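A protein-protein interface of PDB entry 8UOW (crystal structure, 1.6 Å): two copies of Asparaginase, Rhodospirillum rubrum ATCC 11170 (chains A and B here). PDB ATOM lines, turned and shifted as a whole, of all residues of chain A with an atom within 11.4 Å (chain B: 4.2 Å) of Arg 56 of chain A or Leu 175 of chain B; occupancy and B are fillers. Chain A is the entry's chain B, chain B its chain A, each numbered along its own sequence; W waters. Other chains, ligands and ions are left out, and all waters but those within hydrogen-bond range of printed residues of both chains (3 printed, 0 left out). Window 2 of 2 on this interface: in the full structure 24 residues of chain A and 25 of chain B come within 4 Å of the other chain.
The backbone carbonyl oxygen (O) of Arg 56 of chain A lies within hydrogen-bond range of a ring nitrogen (ND1) of His 160 of chain B (2.9 Å).
O of His 160 of chain B sits at hydrogen-bond distance from N of Ala 58 of chain A, 2.9 Å away.
The backbone carbonyl oxygen (O) of Leu 175 of chain B sits at hydrogen-bond distance from the guanidinium group (NH2) of Arg 56 of chain A (3.1 Å).
The guanidinium group (NH1) of Arg 56 of chain A is in hydrogen-bond range of the backbone carbonyl oxygen (O) of Gly 176 of chain B (2.5 Å).
The backbone NH (N) of Leu 175 of chain B lies within hydrogen-bond range of the side-chain amide oxygen (OD1) of Asn 172 of chain B.
His 160 of chain B touches Ala 55 of chain A (CA to O, 3.9 Å).
Arg 56 of chain A touches Met 127 of chain B (NH1 to CG, 3.3 Å).
His 160 of chain B touches Leu 57 of chain A.
Of chain B, only Met 127 (3.3 Å), His 160 (2.9 Å), Leu 175 (3.1 Å) and Gly 176 (2.5 Å) come within 4 Å of Arg 56 of chain A.
Leu 175 of chain B touches just one residue of chain A: Arg 56 (3.1 Å).
Of chain A, only Arg 56 comes within 4 Å of Met 127 of chain B.
Printed residues of chain A within 4 Å of His 160 of chain B: Ala 55, Arg 56, Leu 57 and Ala 58.
No residue of chain A comes within 4 Å of Asn 172 of chain B.
No residue of chain A comes within 4 Å of Gly 174 of chain B.
Gly 176 of chain B touches one residue of chain A.
No residue of chain A comes within 4 Å of Arg 177 of chain B.
Printed residues of chain B within 4 Å of Ala 55 of chain A: His 160.
Of the printed residues of chain B, Ala 58 of chain A touches His 160.
Val 51 of chain A touches none of the printed residues of chain B.
Val 61 of chain A touches none of the printed residues of chain B.
The nearest residue of chain A that does not touch Leu 175 of chain B is Leu 57 of chain A (9.7 Å).
The nearest printed residue of chain B that does not touch Leu 57 of chain A is Arg 177 of chain B (7.4 Å).
Hydrophobic or aromatic side chains of chain A that line the printed part of chain B: Leu 57 and Ala 58.
Along chain A the printed residues that touch a printed residue of chain B span positions 55 to 58.
Of the 8 printed residues of chain B, 4 touch a printed residue of chain A.
Hydrophobic or aromatic side chains of chain B within 4 Å of the printed part of chain A: Met 127 and His 160.
No position is printed for both chains.
Of the 7 pairs that touch across the chains among the printed residues, none has its exchanged pair printed and touching as well.
Water W3 lies within hydrogen-bond range of O of His 160 of chain B (2.7 Å), N of Gly 59 of chain A (2.8 Å) and N of Ala 58 of chain A (3.2 Å).
Water W2 lies within hydrogen-bond range of the backbone carbonyl oxygen of Ala 55 of chain A and the backbone NH of His 160 of chain B.
Water W1 lies within hydrogen-bond range of NH1 of Arg 56 of chain A (3.3 Å) and ND1 of His 160 of chain B (3.5 Å).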
ATOM      1  N   VAL A  48      13.940 -19.131  14.111  1.00  0.00           N
ATOM      2  CA  VAL A  48      13.767 -18.242  12.955  1.00  0.00           C
ATOM      3  C   VAL A  48      15.113 -18.147  12.222  1.00  0.00           C
ATOM      4  O   VAL A  48      15.103 -17.939  11.003  1.00  0.00           O
ATOM      5  CB  VAL A  48      13.243 -16.876  13.416  1.00  0.00           C
ATOM      6  CG1 VAL A  48      14.167 -16.173  14.415  1.00  0.00           C
ATOM      7  CG2 VAL A  48      12.897 -16.014  12.227  1.00  0.00           C
ATOM      8  N   ALA A  49      16.232 -18.210  12.927  1.00  0.00           N
ATOM      9  CA  ALA A  49      17.538 -18.121  12.263  1.00  0.00           C
ATOM     10  C   ALA A  49      17.746 -19.325  11.343  1.00  0.00           C
ATOM     11  O   ALA A  49      18.336 -19.104  10.287  1.00  0.00           O
ATOM     12  CB  ALA A  49      18.613 -17.974  13.321  1.00  0.00           C
ATOM     13  N   GLU A  50      17.272 -20.509  11.729  1.00  0.00           N
ATOM     14  CA  GLU A  50      17.346 -21.718  10.871  1.00  0.00           C
ATOM     15  C   GLU A  50      16.477 -21.531   9.624  1.00  0.00           C
ATOM     16  O   GLU A  50      16.883 -21.851   8.503  1.00  0.00           O
ATOM     17  CB  GLU A  50      16.883 -22.954  11.627  1.00  0.00           C
ATOM     18  CG  GLU A  50      17.701 -23.281  12.844  1.00  0.00           C
ATOM     19  CD  GLU A  50      19.084 -23.797  12.491  1.00  0.00           C
ATOM     20  OE1 GLU A  50      19.503 -23.663  11.315  1.00  0.00           O
ATOM     21  OE2 GLU A  50      19.761 -24.298  13.415  1.00  0.00           O
ATOM     22  N   VAL A  51      15.291 -20.987   9.763  1.00  0.00           N
ATOM     23  CA  VAL A  51      14.374 -20.830   8.616  1.00  0.00           C
ATOM     24  C   VAL A  51      14.931 -19.795   7.628  1.00  0.00           C
ATOM     25  O   VAL A  51      14.887 -20.015   6.386  1.00  0.00           O
ATOM     26  CB  VAL A  51      12.971 -20.453   9.120  1.00  0.00           C
ATOM     27  CG1 VAL A  51      12.067 -20.109   7.954  1.00  0.00           C
ATOM     28  CG2 VAL A  51      12.349 -21.553   9.972  1.00  0.00           C
ATOM     29  N   LEU A  52      15.418 -18.659   8.135  1.00  0.00           N
ATOM     30  CA  LEU A  52      15.890 -17.569   7.251  1.00  0.00           C
ATOM     31  C   LEU A  52      17.185 -17.983   6.514  1.00  0.00           C
ATOM     32  O   LEU A  52      17.326 -17.566   5.364  1.00  0.00           O
ATOM     33  CB  LEU A  52      16.070 -16.318   8.098  1.00  0.00           C
ATOM     34  CG  LEU A  52      14.776 -15.723   8.634  1.00  0.00           C
ATOM     35  CD1 LEU A  52      15.040 -14.331   9.168  1.00  0.00           C
ATOM     36  CD2 LEU A  52      13.677 -15.637   7.601  1.00  0.00           C
ATOM     37  N   LYS A  53      17.938 -18.900   7.081  1.00  0.00           N
ATOM     38  CA  LYS A  53      19.238 -19.389   6.520  1.00  0.00           C
ATOM     39  C   LYS A  53      19.003 -20.074   5.177  1.00  0.00           C
ATOM     40  O   LYS A  53      19.954 -20.024   4.338  1.00  0.00           O
ATOM     41  CB  LYS A  53      19.917 -20.410   7.427  1.00  0.00           C
ATOM     42  CG  LYS A  53      21.033 -21.221   6.753  1.00  0.00           C
ATOM     43  CD  LYS A  53      21.971 -21.899   7.706  1.00  0.00           C
ATOM     44  CE  LYS A  53      23.023 -22.734   6.999  1.00  0.00           C
ATOM     45  NZ  LYS A  53      24.176 -23.017   7.885  1.00  0.00           N
ATOM     46  N   THR A  54      17.904 -20.801   5.043  1.00  0.00           N
ATOM     47  CA  THR A  54      17.570 -21.552   3.795  1.00  0.00           C
ATOM     48  C   THR A  54      16.565 -20.760   2.957  1.00  0.00           C
ATOM     49  O   THR A  54      16.160 -21.257   1.904  1.00  0.00           O
ATOM     50  CB  THR A  54      17.068 -22.949   4.145  1.00  0.00           C
ATOM     51  OG1 THR A  54      15.989 -22.807   5.074  1.00  0.00           O
ATOM     52  CG2 THR A  54      18.178 -23.777   4.748  1.00  0.00           C
ATOM     53  N   ALA A  55      16.147 -19.563   3.389  1.00  0.00           N
ATOM     54  CA  ALA A  55      15.125 -18.787   2.644  1.00  0.00           C
ATOM     55  C   ALA A  55      15.750 -18.041   1.468  1.00  0.00           C
ATOM     56  O   ALA A  55      15.005 -17.412   0.693  1.00  0.00           O
ATOM     57  CB  ALA A  55      14.349 -17.836   3.525  1.00  0.00           C
ATOM     58  N   ARG A  56      17.078 -17.967   1.387  1.00  0.00           N
ATOM     59  CA  ARG A  56      17.755 -17.406   0.203  1.00  0.00           C
ATOM     60  C   ARG A  56      17.310 -15.950   0.074  1.00  0.00           C
ATOM     61  O   ARG A  56      16.831 -15.564  -0.992  1.00  0.00           O
ATOM     62  CB  ARG A  56      17.452 -18.281  -1.017  1.00  0.00           C
ATOM     63  CG  ARG A  56      17.825 -19.739  -0.770  1.00  0.00           C
ATOM     64  CD  ARG A  56      17.539 -20.656  -1.941  1.00  0.00           C
ATOM     65  NE  ARG A  56      18.703 -20.561  -2.814  1.00  0.00           N
ATOM     66  CZ  ARG A  56      18.754 -19.853  -3.926  1.00  0.00           C
ATOM     67  NH1 ARG A  56      17.676 -19.216  -4.346  1.00  0.00           N
ATOM     68  NH2 ARG A  56      19.877 -19.790  -4.629  1.00  0.00           N
ATOM     69  N   LEU A  57      17.387 -15.167   1.147  1.00  0.00           N
ATOM     70  CA  LEU A  57      16.776 -13.813   1.179  1.00  0.00           C
ATOM     71  C   LEU A  57      17.521 -12.826   0.278  1.00  0.00           C
ATOM     72  O   LEU A  57      18.770 -12.922   0.258  1.00  0.00           O
ATOM     73  CB  LEU A  57      16.800 -13.257   2.599  1.00  0.00           C
ATOM     74  CG  LEU A  57      15.962 -14.036   3.613  1.00  0.00           C
ATOM     75  CD1 LEU A  57      16.139 -13.421   4.981  1.00  0.00           C
ATOM     76  CD2 LEU A  57      14.505 -14.076   3.240  1.00  0.00           C
ATOM     77  N   ALA A  58      16.800 -11.886  -0.330  1.00  0.00           N
ATOM     78  CA  ALA A  58      17.419 -10.831  -1.187  1.00  0.00           C
ATOM     79  C   ALA A  58      17.735  -9.580  -0.362  1.00  0.00           C
ATOM     80  O   ALA A  58      18.724  -8.869  -0.710  1.00  0.00           O
ATOM     81  CB  ALA A  58      16.516 -10.504  -2.342  1.00  0.00           C
ATOM     82  N   GLY A  59      16.933  -9.316   0.675  1.00  0.00           N
ATOM     83  CA  GLY A  59      16.855  -8.012   1.347  1.00  0.00           C
ATOM     84  C   GLY A  59      17.693  -7.983   2.602  1.00  0.00           C
ATOM     85  O   GLY A  59      18.292  -9.020   2.954  1.00  0.00           O
ATOM     86  N   ALA A  60      17.679  -6.818   3.260  1.00  0.00           N
ATOM     87  CA  ALA A  60      18.335  -6.538   4.556  1.00  0.00           C
ATOM     88  C   ALA A  60      17.494  -7.155   5.681  1.00  0.00           C
ATOM     89  O   ALA A  60      16.319  -6.715   5.879  1.00  0.00           O
ATOM     90  CB  ALA A  60      18.480  -5.044   4.736  1.00  0.00           C
ATOM     91  N   VAL A  61      18.058  -8.130   6.384  1.00  0.00           N
ATOM     92  CA  VAL A  61      17.394  -8.717   7.594  1.00  0.00           C
ATOM     93  C   VAL A  61      18.450  -8.933   8.653  1.00  0.00           C
ATOM     94  O   VAL A  61      19.510  -9.449   8.289  1.00  0.00           O
ATOM     95  CB  VAL A  61      16.702 -10.062   7.294  1.00  0.00           C
ATOM     96  CG1 VAL A  61      16.012 -10.609   8.530  1.00  0.00           C
ATOM     97  CG2 VAL A  61      15.752  -9.935   6.130  1.00  0.00           C
ATOM     98  N   ILE A 141       6.631 -18.146  10.074  1.00  0.00           N
ATOM     99  CA  ILE A 141       7.743 -17.173   9.894  1.00  0.00           C
ATOM    100  C   ILE A 141       7.630 -16.492   8.520  1.00  0.00           C
ATOM    101  O   ILE A 141       7.722 -15.261   8.431  1.00  0.00           O
ATOM    102  CB  ILE A 141       9.077 -17.903  10.079  1.00  0.00           C
ATOM    103  CG1 ILE A 141       9.310 -18.272  11.545  1.00  0.00           C
ATOM    104  CG2 ILE A 141      10.232 -17.091   9.519  1.00  0.00           C
ATOM    105  CD1 ILE A 141      10.397 -19.261  11.720  1.00  0.00           C
ATOM    106  N   GLY A 142       7.417 -17.237   7.457  1.00  0.00           N
ATOM    107  CA  GLY A 142       7.230 -16.623   6.131  1.00  0.00           C
ATOM    108  C   GLY A 142       6.069 -15.641   6.123  1.00  0.00           C
ATOM    109  O   GLY A 142       6.150 -14.515   5.612  1.00  0.00           O
ATOM    110  N   CYS A 145       6.867 -12.514   8.264  1.00  0.00           N
ATOM    111  CA  CYS A 145       7.850 -11.648   7.559  1.00  0.00           C
ATOM    112  C   CYS A 145       7.139 -10.808   6.526  1.00  0.00           C
ATOM    113  O   CYS A 145       7.323  -9.553   6.524  1.00  0.00           O
ATOM    114  CB  CYS A 145       9.010 -12.422   6.954  1.00  0.00           C
ATOM    115  SG  CYS A 145      10.201 -13.059   8.153  1.00  0.00           S
ATOM    116  N   MET B 127      13.411 -23.124  -5.050  1.00  0.00           N
ATOM    117  CA  MET B 127      14.652 -23.461  -5.756  1.00  0.00           C
ATOM    118  C   MET B 127      15.124 -24.853  -5.345  1.00  0.00           C
ATOM    119  O   MET B 127      15.900 -25.485  -6.139  1.00  0.00           O
ATOM    120  CB  MET B 127      15.707 -22.407  -5.443  1.00  0.00           C
ATOM    121  CG  MET B 127      15.266 -21.006  -5.803  1.00  0.00           C
ATOM    122  SD  MET B 127      14.989 -20.869  -7.607  1.00  0.00           S
ATOM    123  CE  MET B 127      14.397 -19.176  -7.718  1.00  0.00           C
ATOM    124  N   HIS B 160      12.528 -15.128  -2.217  1.00  0.00           N
ATOM    125  CA  HIS B 160      13.684 -14.504  -1.525  1.00  0.00           C
ATOM    126  C   HIS B 160      13.228 -13.462  -0.499  1.00  0.00           C
ATOM    127  O   HIS B 160      13.929 -12.496  -0.179  1.00  0.00           O
ATOM    128  CB  HIS B 160      14.632 -13.782  -2.522  1.00  0.00           C
ATOM    129  CG  HIS B 160      14.919 -14.650  -3.703  1.00  0.00           C
ATOM    130  ND1 HIS B 160      15.545 -15.873  -3.581  1.00  0.00           N
ATOM    131  CD2 HIS B 160      14.657 -14.479  -5.032  1.00  0.00           C
ATOM    132  CE1 HIS B 160      15.680 -16.410  -4.793  1.00  0.00           C
ATOM    133  NE2 HIS B 160      15.077 -15.616  -5.679  1.00  0.00           N
ATOM    134  N   ASN B 172      17.805 -15.553 -12.870  1.00  0.00           N
ATOM    135  CA  ASN B 172      19.246 -15.906 -12.995  1.00  0.00           C
ATOM    136  C   ASN B 172      19.401 -17.414 -12.725  1.00  0.00           C
ATOM    137  O   ASN B 172      19.425 -17.833 -11.542  1.00  0.00           O
ATOM    138  CB  ASN B 172      20.104 -15.010 -12.105  1.00  0.00           C
ATOM    139  CG  ASN B 172      21.577 -15.324 -12.241  1.00  0.00           C
ATOM    140  OD1 ASN B 172      21.932 -16.447 -12.562  1.00  0.00           O
ATOM    141  ND2 ASN B 172      22.434 -14.376 -11.915  1.00  0.00           N
ATOM    142  N   ARG B 173      19.541 -18.220 -13.785  1.00  0.00           N
ATOM    143  CA  ARG B 173      19.668 -19.699 -13.682  1.00  0.00           C
ATOM    144  C   ARG B 173      20.915 -20.083 -12.878  1.00  0.00           C
ATOM    145  O   ARG B 173      20.787 -20.946 -11.989  1.00  0.00           O
ATOM    146  CB  ARG B 173      19.679 -20.329 -15.074  1.00  0.00           C
ATOM    147  CG  ARG B 173      18.383 -20.110 -15.838  1.00  0.00           C
ATOM    148  CD  ARG B 173      18.317 -20.980 -17.075  1.00  0.00           C
ATOM    149  NE  ARG B 173      17.092 -20.724 -17.817  1.00  0.00           N
ATOM    150  CZ  ARG B 173      16.891 -21.053 -19.092  1.00  0.00           C
ATOM    151  NH1 ARG B 173      17.842 -21.655 -19.793  1.00  0.00           N
ATOM    152  NH2 ARG B 173      15.729 -20.776 -19.664  1.00  0.00           N
ATOM    153  N   GLY B 174      22.067 -19.462 -13.148  1.00  0.00           N
ATOM    154  CA  GLY B 174      23.338 -19.795 -12.475  1.00  0.00           C
ATOM    155  C   GLY B 174      23.265 -19.654 -10.962  1.00  0.00           C
ATOM    156  O   GLY B 174      23.750 -20.560 -10.257  1.00  0.00           O
ATOM    157  N   LEU B 175      22.674 -18.560 -10.470  1.00  0.00           N
ATOM    158  CA  LEU B 175      22.633 -18.205  -9.023  1.00  0.00           C
ATOM    159  C   LEU B 175      21.374 -18.747  -8.347  1.00  0.00           C
ATOM    160  O   LEU B 175      21.325 -18.694  -7.098  1.00  0.00           O
ATOM    161  CB  LEU B 175      22.708 -16.688  -8.881  1.00  0.00           C
ATOM    162  CG  LEU B 175      24.092 -16.090  -9.105  1.00  0.00           C
ATOM    163  CD1 LEU B 175      24.104 -14.634  -8.674  1.00  0.00           C
ATOM    164  CD2 LEU B 175      25.149 -16.887  -8.366  1.00  0.00           C
ATOM    165  N   GLY B 176      20.436 -19.304  -9.122  1.00  0.00           N
ATOM    166  CA  GLY B 176      19.151 -19.814  -8.603  1.00  0.00           C
ATOM    167  C   GLY B 176      18.396 -18.690  -7.916  1.00  0.00           C
ATOM    168  O   GLY B 176      17.950 -18.875  -6.785  1.00  0.00           O
ATOM    169  N   ARG B 177      18.288 -17.523  -8.540  1.00  0.00           N
ATOM    170  CA  ARG B 177      17.593 -16.382  -7.907  1.00  0.00           C
ATOM    171  C   ARG B 177      16.901 -15.508  -8.955  1.00  0.00           C
ATOM    172  O   ARG B 177      17.360 -15.401 -10.099  1.00  0.00           O
ATOM    173  CB  ARG B 177      18.589 -15.609  -7.039  1.00  0.00           C
ATOM    174  CG  ARG B 177      19.462 -14.642  -7.808  1.00  0.00           C
ATOM    175  CD  ARG B 177      20.437 -13.922  -6.900  1.00  0.00           C
ATOM    176  NE  ARG B 177      21.138 -12.907  -7.671  1.00  0.00           N
ATOM    177  CZ  ARG B 177      22.147 -12.166  -7.228  1.00  0.00           C
ATOM    178  NH1 ARG B 177      22.618 -12.335  -6.006  1.00  0.00           N
ATOM    179  NH2 ARG B 177      22.700 -11.274  -8.027  1.00  0.00           N
HETATM  180  O   HOH W   1      14.636 -19.193  -3.127  1.00  0.00           O
HETATM  181  O   HOH W   2      13.145 -17.762  -1.273  1.00  0.00           O
HETATM  182  O   HOH W   3      14.599 -10.527   1.583  1.00  0.00           O
